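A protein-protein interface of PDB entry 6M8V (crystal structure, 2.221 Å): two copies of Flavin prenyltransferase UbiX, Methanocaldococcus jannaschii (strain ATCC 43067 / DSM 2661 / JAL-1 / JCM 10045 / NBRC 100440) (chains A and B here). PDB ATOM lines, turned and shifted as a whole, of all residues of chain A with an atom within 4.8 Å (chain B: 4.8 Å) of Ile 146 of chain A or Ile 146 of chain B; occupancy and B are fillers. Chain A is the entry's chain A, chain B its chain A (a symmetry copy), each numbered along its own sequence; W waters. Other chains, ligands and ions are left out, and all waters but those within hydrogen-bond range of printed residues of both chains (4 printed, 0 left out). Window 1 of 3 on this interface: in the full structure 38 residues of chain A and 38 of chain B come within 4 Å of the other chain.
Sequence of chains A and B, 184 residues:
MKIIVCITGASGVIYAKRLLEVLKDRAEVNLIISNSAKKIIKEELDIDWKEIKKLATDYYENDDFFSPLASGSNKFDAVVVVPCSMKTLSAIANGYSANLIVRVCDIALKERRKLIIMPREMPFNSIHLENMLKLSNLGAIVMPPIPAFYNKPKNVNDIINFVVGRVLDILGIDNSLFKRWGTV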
ATOM      1  N   PRO A 119     -15.795 -15.064   3.844  1.00  0.00           N
ATOM      2  CA  PRO A 119     -15.581 -15.814   2.598  1.00  0.00           C
ATOM      3  C   PRO A 119     -14.103 -15.870   2.231  1.00  0.00           C
ATOM      4  O   PRO A 119     -13.419 -14.846   2.193  1.00  0.00           O
ATOM      5  CB  PRO A 119     -16.394 -15.024   1.565  1.00  0.00           C
ATOM      6  CG  PRO A 119     -16.457 -13.646   2.126  1.00  0.00           C
ATOM      7  CD  PRO A 119     -16.503 -13.793   3.616  1.00  0.00           C
ATOM      8  N   ARG A 120     -13.617 -17.080   1.955  1.00  0.00           N
ATOM      9  CA  ARG A 120     -12.210 -17.335   1.652  1.00  0.00           C
ATOM     10  C   ARG A 120     -12.108 -17.817   0.212  1.00  0.00           C
ATOM     11  O   ARG A 120     -12.460 -18.964  -0.094  1.00  0.00           O
ATOM     12  CB  ARG A 120     -11.620 -18.367   2.615  1.00  0.00           C
ATOM     13  CG  ARG A 120     -10.183 -18.091   3.108  1.00  0.00           C
ATOM     14  CD  ARG A 120      -9.133 -18.072   1.981  1.00  0.00           C
ATOM     15  NE  ARG A 120      -9.337 -19.120   0.990  1.00  0.00           N
ATOM     16  CZ  ARG A 120      -8.673 -19.215  -0.157  1.00  0.00           C
ATOM     17  NH1 ARG A 120      -7.745 -18.322  -0.470  1.00  0.00           N
ATOM     18  NH2 ARG A 120      -8.953 -20.200  -1.003  1.00  0.00           N
ATOM     19  N   GLU A 121     -11.620 -16.945  -0.663  1.00  0.00           N
ATOM     20  CA  GLU A 121     -11.456 -17.258  -2.073  1.00  0.00           C
ATOM     21  C   GLU A 121     -10.530 -16.217  -2.679  1.00  0.00           C
ATOM     22  O   GLU A 121     -10.461 -15.080  -2.202  1.00  0.00           O
ATOM     23  CB  GLU A 121     -12.802 -17.274  -2.813  1.00  0.00           C
ATOM     24  CG  GLU A 121     -12.721 -17.769  -4.252  1.00  0.00           C
ATOM     25  CD  GLU A 121     -11.943 -19.072  -4.368  1.00  0.00           C
ATOM     26  OE1 GLU A 121     -10.700 -19.018  -4.522  1.00  0.00           O
ATOM     27  OE2 GLU A 121     -12.574 -20.151  -4.305  1.00  0.00           O
ATOM     28  N   MET A 122      -9.827 -16.613  -3.731  1.00  0.00           N
ATOM     29  CA  MET A 122      -8.928 -15.676  -4.380  1.00  0.00           C
ATOM     30  C   MET A 122      -8.593 -16.175  -5.780  1.00  0.00           C
ATOM     31  O   MET A 122      -8.126 -17.310  -5.940  1.00  0.00           O
ATOM     32  CB  MET A 122      -7.667 -15.498  -3.537  1.00  0.00           C
ATOM     33  CG  MET A 122      -6.755 -14.390  -3.996  1.00  0.00           C
ATOM     34  SD  MET A 122      -5.237 -14.367  -3.019  1.00  0.00           S
ATOM     35  CE  MET A 122      -4.326 -13.127  -3.910  1.00  0.00           C
ATOM     36  N   PHE A 124     -11.888 -13.295  -6.330  1.00  0.00           N
ATOM     37  CA  PHE A 124     -13.345 -13.336  -6.366  1.00  0.00           C
ATOM     38  C   PHE A 124     -13.827 -13.076  -7.789  1.00  0.00           C
ATOM     39  O   PHE A 124     -13.229 -12.290  -8.529  1.00  0.00           O
ATOM     40  CB  PHE A 124     -13.951 -12.274  -5.444  1.00  0.00           C
ATOM     41  CG  PHE A 124     -13.796 -12.559  -3.973  1.00  0.00           C
ATOM     42  CD1 PHE A 124     -14.203 -13.768  -3.435  1.00  0.00           C
ATOM     43  CD2 PHE A 124     -13.270 -11.598  -3.125  1.00  0.00           C
ATOM     44  CE1 PHE A 124     -14.079 -14.024  -2.082  1.00  0.00           C
ATOM     45  CE2 PHE A 124     -13.142 -11.846  -1.769  1.00  0.00           C
ATOM     46  CZ  PHE A 124     -13.550 -13.062  -1.247  1.00  0.00           C
ATOM     47  N   PRO A 144     -14.044 -11.238   4.767  1.00  0.00           N
ATOM     48  CA  PRO A 144     -13.035 -12.200   4.282  1.00  0.00           C
ATOM     49  C   PRO A 144     -11.749 -12.065   5.075  1.00  0.00           C
ATOM     50  O   PRO A 144     -11.346 -10.948   5.433  1.00  0.00           O
ATOM     51  CB  PRO A 144     -12.828 -11.803   2.808  1.00  0.00           C
ATOM     52  CG  PRO A 144     -13.488 -10.469   2.646  1.00  0.00           C
ATOM     53  CD  PRO A 144     -14.553 -10.376   3.687  1.00  0.00           C
ATOM     54  N   PRO A 145     -11.086 -13.178   5.384  1.00  0.00           N
ATOM     55  CA  PRO A 145      -9.860 -13.100   6.195  1.00  0.00           C
ATOM     56  C   PRO A 145      -8.714 -12.479   5.416  1.00  0.00           C
ATOM     57  O   PRO A 145      -8.005 -13.163   4.673  1.00  0.00           O
ATOM     58  CB  PRO A 145      -9.580 -14.565   6.558  1.00  0.00           C
ATOM     59  CG  PRO A 145     -10.205 -15.359   5.438  1.00  0.00           C
ATOM     60  CD  PRO A 145     -11.412 -14.559   4.979  1.00  0.00           C
ATOM     61  N   ILE A 146      -8.546 -11.170   5.569  1.00  0.00           N
ATOM     62  CA  ILE A 146      -7.526 -10.418   4.846  1.00  0.00           C
ATOM     63  C   ILE A 146      -6.595  -9.782   5.871  1.00  0.00           C
ATOM     64  O   ILE A 146      -6.840  -8.653   6.327  1.00  0.00           O
ATOM     65  CB  ILE A 146      -8.158  -9.368   3.922  1.00  0.00           C
ATOM     66  CG1 ILE A 146      -9.301 -10.003   3.128  1.00  0.00           C
ATOM     67  CG2 ILE A 146      -7.116  -8.803   2.982  1.00  0.00           C
ATOM     68  CD1 ILE A 146     -10.035  -9.050   2.222  1.00  0.00           C
ATOM     69  N   PRO A 147      -5.532 -10.473   6.269  1.00  0.00           N
ATOM     70  CA  PRO A 147      -4.641  -9.923   7.294  1.00  0.00           C
ATOM     71  C   PRO A 147      -4.000  -8.619   6.848  1.00  0.00           C
ATOM     72  O   PRO A 147      -3.775  -8.382   5.658  1.00  0.00           O
ATOM     73  CB  PRO A 147      -3.593 -11.025   7.486  1.00  0.00           C
ATOM     74  CG  PRO A 147      -3.712 -11.911   6.288  1.00  0.00           C
ATOM     75  CD  PRO A 147      -5.134 -11.823   5.840  1.00  0.00           C
ATOM     76  N   ALA A 148      -3.751  -7.755   7.826  1.00  0.00           N
ATOM     77  CA  ALA A 148      -2.916  -6.575   7.665  1.00  0.00           C
ATOM     78  C   ALA A 148      -1.531  -6.856   8.239  1.00  0.00           C
ATOM     79  O   ALA A 148      -1.283  -7.902   8.842  1.00  0.00           O
ATOM     80  CB  ALA A 148      -3.550  -5.365   8.350  1.00  0.00           C
ATOM     81  N   PHE A 162      -4.379 -11.768  14.499  1.00  0.00           N
ATOM     82  CA  PHE A 162      -4.934 -10.511  14.003  1.00  0.00           C
ATOM     83  C   PHE A 162      -6.351 -10.716  13.480  1.00  0.00           C
ATOM     84  O   PHE A 162      -7.282  -9.993  13.862  1.00  0.00           O
ATOM     85  CB  PHE A 162      -4.041  -9.927  12.903  1.00  0.00           C
ATOM     86  CG  PHE A 162      -4.607  -8.684  12.264  1.00  0.00           C
ATOM     87  CD1 PHE A 162      -4.303  -7.433  12.771  1.00  0.00           C
ATOM     88  CD2 PHE A 162      -5.453  -8.768  11.164  1.00  0.00           C
ATOM     89  CE1 PHE A 162      -4.825  -6.292  12.197  1.00  0.00           C
ATOM     90  CE2 PHE A 162      -5.982  -7.631  10.588  1.00  0.00           C
ATOM     91  CZ  PHE A 162      -5.666  -6.389  11.105  1.00  0.00           C
ATOM     92  N   PRO B 119      -7.617  -5.271  -3.272  1.00  0.00           N
ATOM     93  CA  PRO B 119      -8.096  -4.412  -2.179  1.00  0.00           C
ATOM     94  C   PRO B 119      -7.865  -5.062  -0.820  1.00  0.00           C
ATOM     95  O   PRO B 119      -8.232  -6.217  -0.598  1.00  0.00           O
ATOM     96  CB  PRO B 119      -9.589  -4.248  -2.486  1.00  0.00           C
ATOM     97  CG  PRO B 119      -9.933  -5.458  -3.283  1.00  0.00           C
ATOM     98  CD  PRO B 119      -8.721  -5.794  -4.096  1.00  0.00           C
ATOM     99  N   ARG B 120      -7.255  -4.305   0.091  1.00  0.00           N
ATOM    100  CA  ARG B 120      -6.889  -4.783   1.423  1.00  0.00           C
ATOM    101  C   ARG B 120      -7.701  -4.008   2.452  1.00  0.00           C
ATOM    102  O   ARG B 120      -7.422  -2.831   2.715  1.00  0.00           O
ATOM    103  CB  ARG B 120      -5.389  -4.615   1.674  1.00  0.00           C
ATOM    104  CG  ARG B 120      -4.692  -5.773   2.420  1.00  0.00           C
ATOM    105  CD  ARG B 120      -5.228  -6.005   3.845  1.00  0.00           C
ATOM    106  NE  ARG B 120      -5.483  -4.767   4.570  1.00  0.00           N
ATOM    107  CZ  ARG B 120      -6.097  -4.693   5.746  1.00  0.00           C
ATOM    108  NH1 ARG B 120      -6.525  -5.793   6.349  1.00  0.00           N
ATOM    109  NH2 ARG B 120      -6.300  -3.508   6.311  1.00  0.00           N
ATOM    110  N   GLU B 121      -8.693  -4.671   3.034  1.00  0.00           N
ATOM    111  CA  GLU B 121      -9.553  -4.071   4.040  1.00  0.00           C
ATOM    112  C   GLU B 121     -10.289  -5.190   4.757  1.00  0.00           C
ATOM    113  O   GLU B 121     -10.522  -6.259   4.184  1.00  0.00           O
ATOM    114  CB  GLU B 121     -10.554  -3.085   3.418  1.00  0.00           C
ATOM    115  CG  GLU B 121     -11.365  -2.288   4.434  1.00  0.00           C
ATOM    116  CD  GLU B 121     -10.485  -1.670   5.512  1.00  0.00           C
ATOM    117  OE1 GLU B 121     -10.228  -2.345   6.537  1.00  0.00           O
ATOM    118  OE2 GLU B 121     -10.051  -0.510   5.334  1.00  0.00           O
ATOM    119  N   MET B 122     -10.651  -4.935   6.006  1.00  0.00           N
ATOM    120  CA  MET B 122     -11.371  -5.946   6.759  1.00  0.00           C
ATOM    121  C   MET B 122     -12.067  -5.298   7.950  1.00  0.00           C
ATOM    122  O   MET B 122     -11.415  -4.626   8.759  1.00  0.00           O
ATOM    123  CB  MET B 122     -10.409  -7.044   7.207  1.00  0.00           C
ATOM    124  CG  MET B 122     -11.072  -8.254   7.810  1.00  0.00           C
ATOM    125  SD  MET B 122      -9.837  -9.415   8.431  1.00  0.00           S
ATOM    126  CE  MET B 122     -10.905 -10.591   9.231  1.00  0.00           C
ATOM    127  N   PHE B 124     -15.144  -5.544   4.800  1.00  0.00           N
ATOM    128  CA  PHE B 124     -15.626  -4.702   3.712  1.00  0.00           C
ATOM    129  C   PHE B 124     -17.021  -4.185   4.045  1.00  0.00           C
ATOM    130  O   PHE B 124     -17.827  -4.886   4.664  1.00  0.00           O
ATOM    131  CB  PHE B 124     -15.696  -5.485   2.397  1.00  0.00           C
ATOM    132  CG  PHE B 124     -14.357  -5.817   1.794  1.00  0.00           C
ATOM    133  CD1 PHE B 124     -13.413  -4.830   1.568  1.00  0.00           C
ATOM    134  CD2 PHE B 124     -14.059  -7.118   1.424  1.00  0.00           C
ATOM    135  CE1 PHE B 124     -12.190  -5.131   0.996  1.00  0.00           C
ATOM    136  CE2 PHE B 124     -12.837  -7.428   0.852  1.00  0.00           C
ATOM    137  CZ  PHE B 124     -11.901  -6.431   0.636  1.00  0.00           C
ATOM    138  N   PRO B 144      -8.433  -9.484  -3.651  1.00  0.00           N
ATOM    139  CA  PRO B 144      -7.949  -9.139  -2.300  1.00  0.00           C
ATOM    140  C   PRO B 144      -6.993 -10.201  -1.792  1.00  0.00           C
ATOM    141  O   PRO B 144      -7.198 -11.400  -2.035  1.00  0.00           O
ATOM    142  CB  PRO B 144      -9.234  -9.090  -1.452  1.00  0.00           C
ATOM    143  CG  PRO B 144     -10.305  -9.709  -2.295  1.00  0.00           C
ATOM    144  CD  PRO B 144      -9.903  -9.528  -3.721  1.00  0.00           C
ATOM    145  N   PRO B 145      -5.928  -9.802  -1.098  1.00  0.00           N
ATOM    146  CA  PRO B 145      -4.946 -10.793  -0.627  1.00  0.00           C
ATOM    147  C   PRO B 145      -5.513 -11.653   0.488  1.00  0.00           C
ATOM    148  O   PRO B 145      -5.478 -11.277   1.663  1.00  0.00           O
ATOM    149  CB  PRO B 145      -3.772  -9.929  -0.147  1.00  0.00           C
ATOM    150  CG  PRO B 145      -4.403  -8.615   0.245  1.00  0.00           C
ATOM    151  CD  PRO B 145      -5.589  -8.426  -0.685  1.00  0.00           C
ATOM    152  N   ILE B 146      -6.057 -12.806   0.117  1.00  0.00           N
ATOM    153  CA  ILE B 146      -6.693 -13.717   1.062  1.00  0.00           C
ATOM    154  C   ILE B 146      -5.949 -15.046   1.009  1.00  0.00           C
ATOM    155  O   ILE B 146      -6.297 -15.930   0.209  1.00  0.00           O
ATOM    156  CB  ILE B 146      -8.187 -13.889   0.752  1.00  0.00           C
ATOM    157  CG1 ILE B 146      -8.823 -12.518   0.513  1.00  0.00           C
ATOM    158  CG2 ILE B 146      -8.880 -14.598   1.895  1.00  0.00           C
ATOM    159  CD1 ILE B 146     -10.283 -12.564   0.146  1.00  0.00           C
ATOM    160  N   PRO B 147      -4.916 -15.221   1.828  1.00  0.00           N
ATOM    161  CA  PRO B 147      -4.138 -16.461   1.772  1.00  0.00           C
ATOM    162  C   PRO B 147      -4.987 -17.679   2.097  1.00  0.00           C
ATOM    163  O   PRO B 147      -5.959 -17.606   2.853  1.00  0.00           O
ATOM    164  CB  PRO B 147      -3.044 -16.244   2.823  1.00  0.00           C
ATOM    165  CG  PRO B 147      -3.519 -15.112   3.676  1.00  0.00           C
ATOM    166  CD  PRO B 147      -4.376 -14.258   2.801  1.00  0.00           C
ATOM    167  N   ALA B 148      -4.627 -18.795   1.473  1.00  0.00           N
ATOM    168  CA  ALA B 148      -5.125 -20.114   1.829  1.00  0.00           C
ATOM    169  C   ALA B 148      -4.076 -20.839   2.668  1.00  0.00           C
ATOM    170  O   ALA B 148      -2.958 -20.358   2.858  1.00  0.00           O
ATOM    171  CB  ALA B 148      -5.468 -20.920   0.577  1.00  0.00           C
ATOM    172  N   PHE B 162       2.506 -17.470  -1.424  1.00  0.00           N
ATOM    173  CA  PHE B 162       1.254 -17.980  -1.977  1.00  0.00           C
ATOM    174  C   PHE B 162       0.501 -16.879  -2.714  1.00  0.00           C
ATOM    175  O   PHE B 162       0.095 -17.048  -3.872  1.00  0.00           O
ATOM    176  CB  PHE B 162       0.379 -18.572  -0.868  1.00  0.00           C
ATOM    177  CG  PHE B 162      -0.979 -19.019  -1.345  1.00  0.00           C
ATOM    178  CD1 PHE B 162      -1.176 -20.315  -1.790  1.00  0.00           C
ATOM    179  CD2 PHE B 162      -2.057 -18.141  -1.361  1.00  0.00           C
ATOM    180  CE1 PHE B 162      -2.414 -20.728  -2.237  1.00  0.00           C
ATOM    181  CE2 PHE B 162      -3.296 -18.547  -1.812  1.00  0.00           C
ATOM    182  CZ  PHE B 162      -3.476 -19.845  -2.250  1.00  0.00           C
HETATM  183  O   HOH W   1      -6.697 -15.672   4.929  1.00  0.00           O
HETATM  184  O   HOH W   2     -12.434  -8.319   4.797  1.00  0.00           O
HETATM  185  O   HOH W   3      -9.484 -12.634  -3.358  1.00  0.00           O
HETATM  186  O   HOH W   4      -3.478 -10.135   3.327  1.00  0.00           O
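Of the printed residues of chain B, Ile 146 of chain A touches Arg 120 (2.9 Å), Glu 121 (3.4 Å), Met 122 (3.6 Å), Phe 124 (3.5 Å), Pro 144 (3.8 Å), Pro 145 (3.2 Å) and Ile 146 (3.7 Å).
Ile 146 of chain B touches just these residues of chain A: Arg 120 (2.9 Å), Glu 121 (3.4 Å), Met 122 (3.6 Å), Phe 124 (3.5 Å), Pro 144 (3.8 Å), Pro 145 (3.2 Å) and Ile 146 (3.7 Å).
Printed residues of chain A within 4 Å of Glu 121 of chain B: Ile 146 (3.4 Å).
Of the printed residues of chain B, Phe 124 of chain A touches Pro 144 and Ile 146.
Of the printed residues of chain B, Arg 120 of chain A touches Ile 146, Pro 147 and Ala 148.
Printed residues of chain B within 4 Å of Met 122 of chain A: Pro 144 and Ile 146.
Water W1 bridges O of Pro 145 of chain A (2.8 Å) and O of Pro 147 of chain B (2.9 Å).
Water W4 bridges the backbone carbonyl oxygen of Pro 145 of chain B (2.8 Å) and the backbone carbonyl oxygen of Pro 147 of chain A (2.9 Å).
Water W3 bridges the backbone carbonyl oxygen (O) of Glu 121 of chain A (2.9 Å) and the backbone carbonyl oxygen (O) of Pro 144 of chain B (2.9 Å).
Water W2 bridges the backbone carbonyl oxygen (O) of Glu 121 of chain B (2.9 Å) and the backbone carbonyl oxygen (O) of Pro 144 of chain A (2.9 Å).
Glu 121 of chain A touches Ile 146 of chain B (O to CD1, 3.4 Å).
CE2 of Phe 124 of chain A touches CD1 of Ile 146 of chain B, 3.5 Å away.
Phe 124 of chain B touches Pro 144 of chain A (CE2 to CG, 3.6 Å).
Ile 146 of chain B touches Pro 144 of chain A (CD1 to CB, 3.8 Å).
O of Pro 145 of chain A touches CG2 of Ile 146 of chain B (3.2 Å).
Glu 121 of chain B touches Ile 146 of chain A (O to CD1, 3.4 Å).
CE2 of Phe 124 of chain B touches CD1 of Ile 146 of chain A, 3.5 Å away.
CB of Pro 144 of chain B touches CD1 of Ile 146 of chain A, 3.8 Å away.
O of Pro 145 of chain B touches CG2 of Ile 146 of chain A (3.2 Å).
NH1 of Arg 120 of chain B touches CB of Ala 148 of chain A (3.6 Å).
Met 122 of chain A touches Pro 144 of chain B, and with the chains exchanged Pro 144 of chain A touches Met 122 of chain B.
Met 122 of chain A touches Ile 146 of chain B, and with the chains exchanged Ile 146 of chain A touches Met 122 of chain B.
Phe 124 of chain A touches Pro 144 of chain B, and with the chains exchanged Pro 144 of chain A touches Phe 124 of chain B.
Ile 146 of chain A touches its own counterpart, Ile 146 of chain B.
Of the 22 pairs that touch across the chains among the printed residues, 22 have their exchanged pair printed and touching as well.
SD of Met 122 of chain A sits at hydrogen-bond distance from N of Ile 146 of chain B (3.6 Å).
O of Pro 144 of chain B lies close to SD of Met 122 of chain A (3.7 Å).
N of Ile 146 of chain A lies within hydrogen-bond range of SD of Met 122 of chain B (3.6 Å).
The backbone carbonyl oxygen (O) of Pro 144 of chain A lies close to the side-chain sulfur (SD) of Met 122 of chain B, 3.7 Å away.
The guanidinium group of Arg 120 of chain B lies within hydrogen-bond range of the backbone carbonyl oxygen of Ile 146 of chain A.
The guanidinium group (NH1) of Arg 120 of chain A is in hydrogen-bond range of the backbone carbonyl oxygen (O) of Ile 146 of chain B, 2.9 Å away.
Of the 11 printed residues of chain B, 9 touch a printed residue of chain A.
Hydrophobic or aromatic side chains of chain B within 4 Å of the printed part of chain A: Met 122, Phe 124, Pro 144, Pro 145, Ile 146, Pro 147 and Ala 148.
Among the printed residues, 22 pairs touch across the chains.
Among the printed residues, no Asp or Glu carboxylate lies within 4 Å of a Lys or Arg side-chain nitrogen of the other chain.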
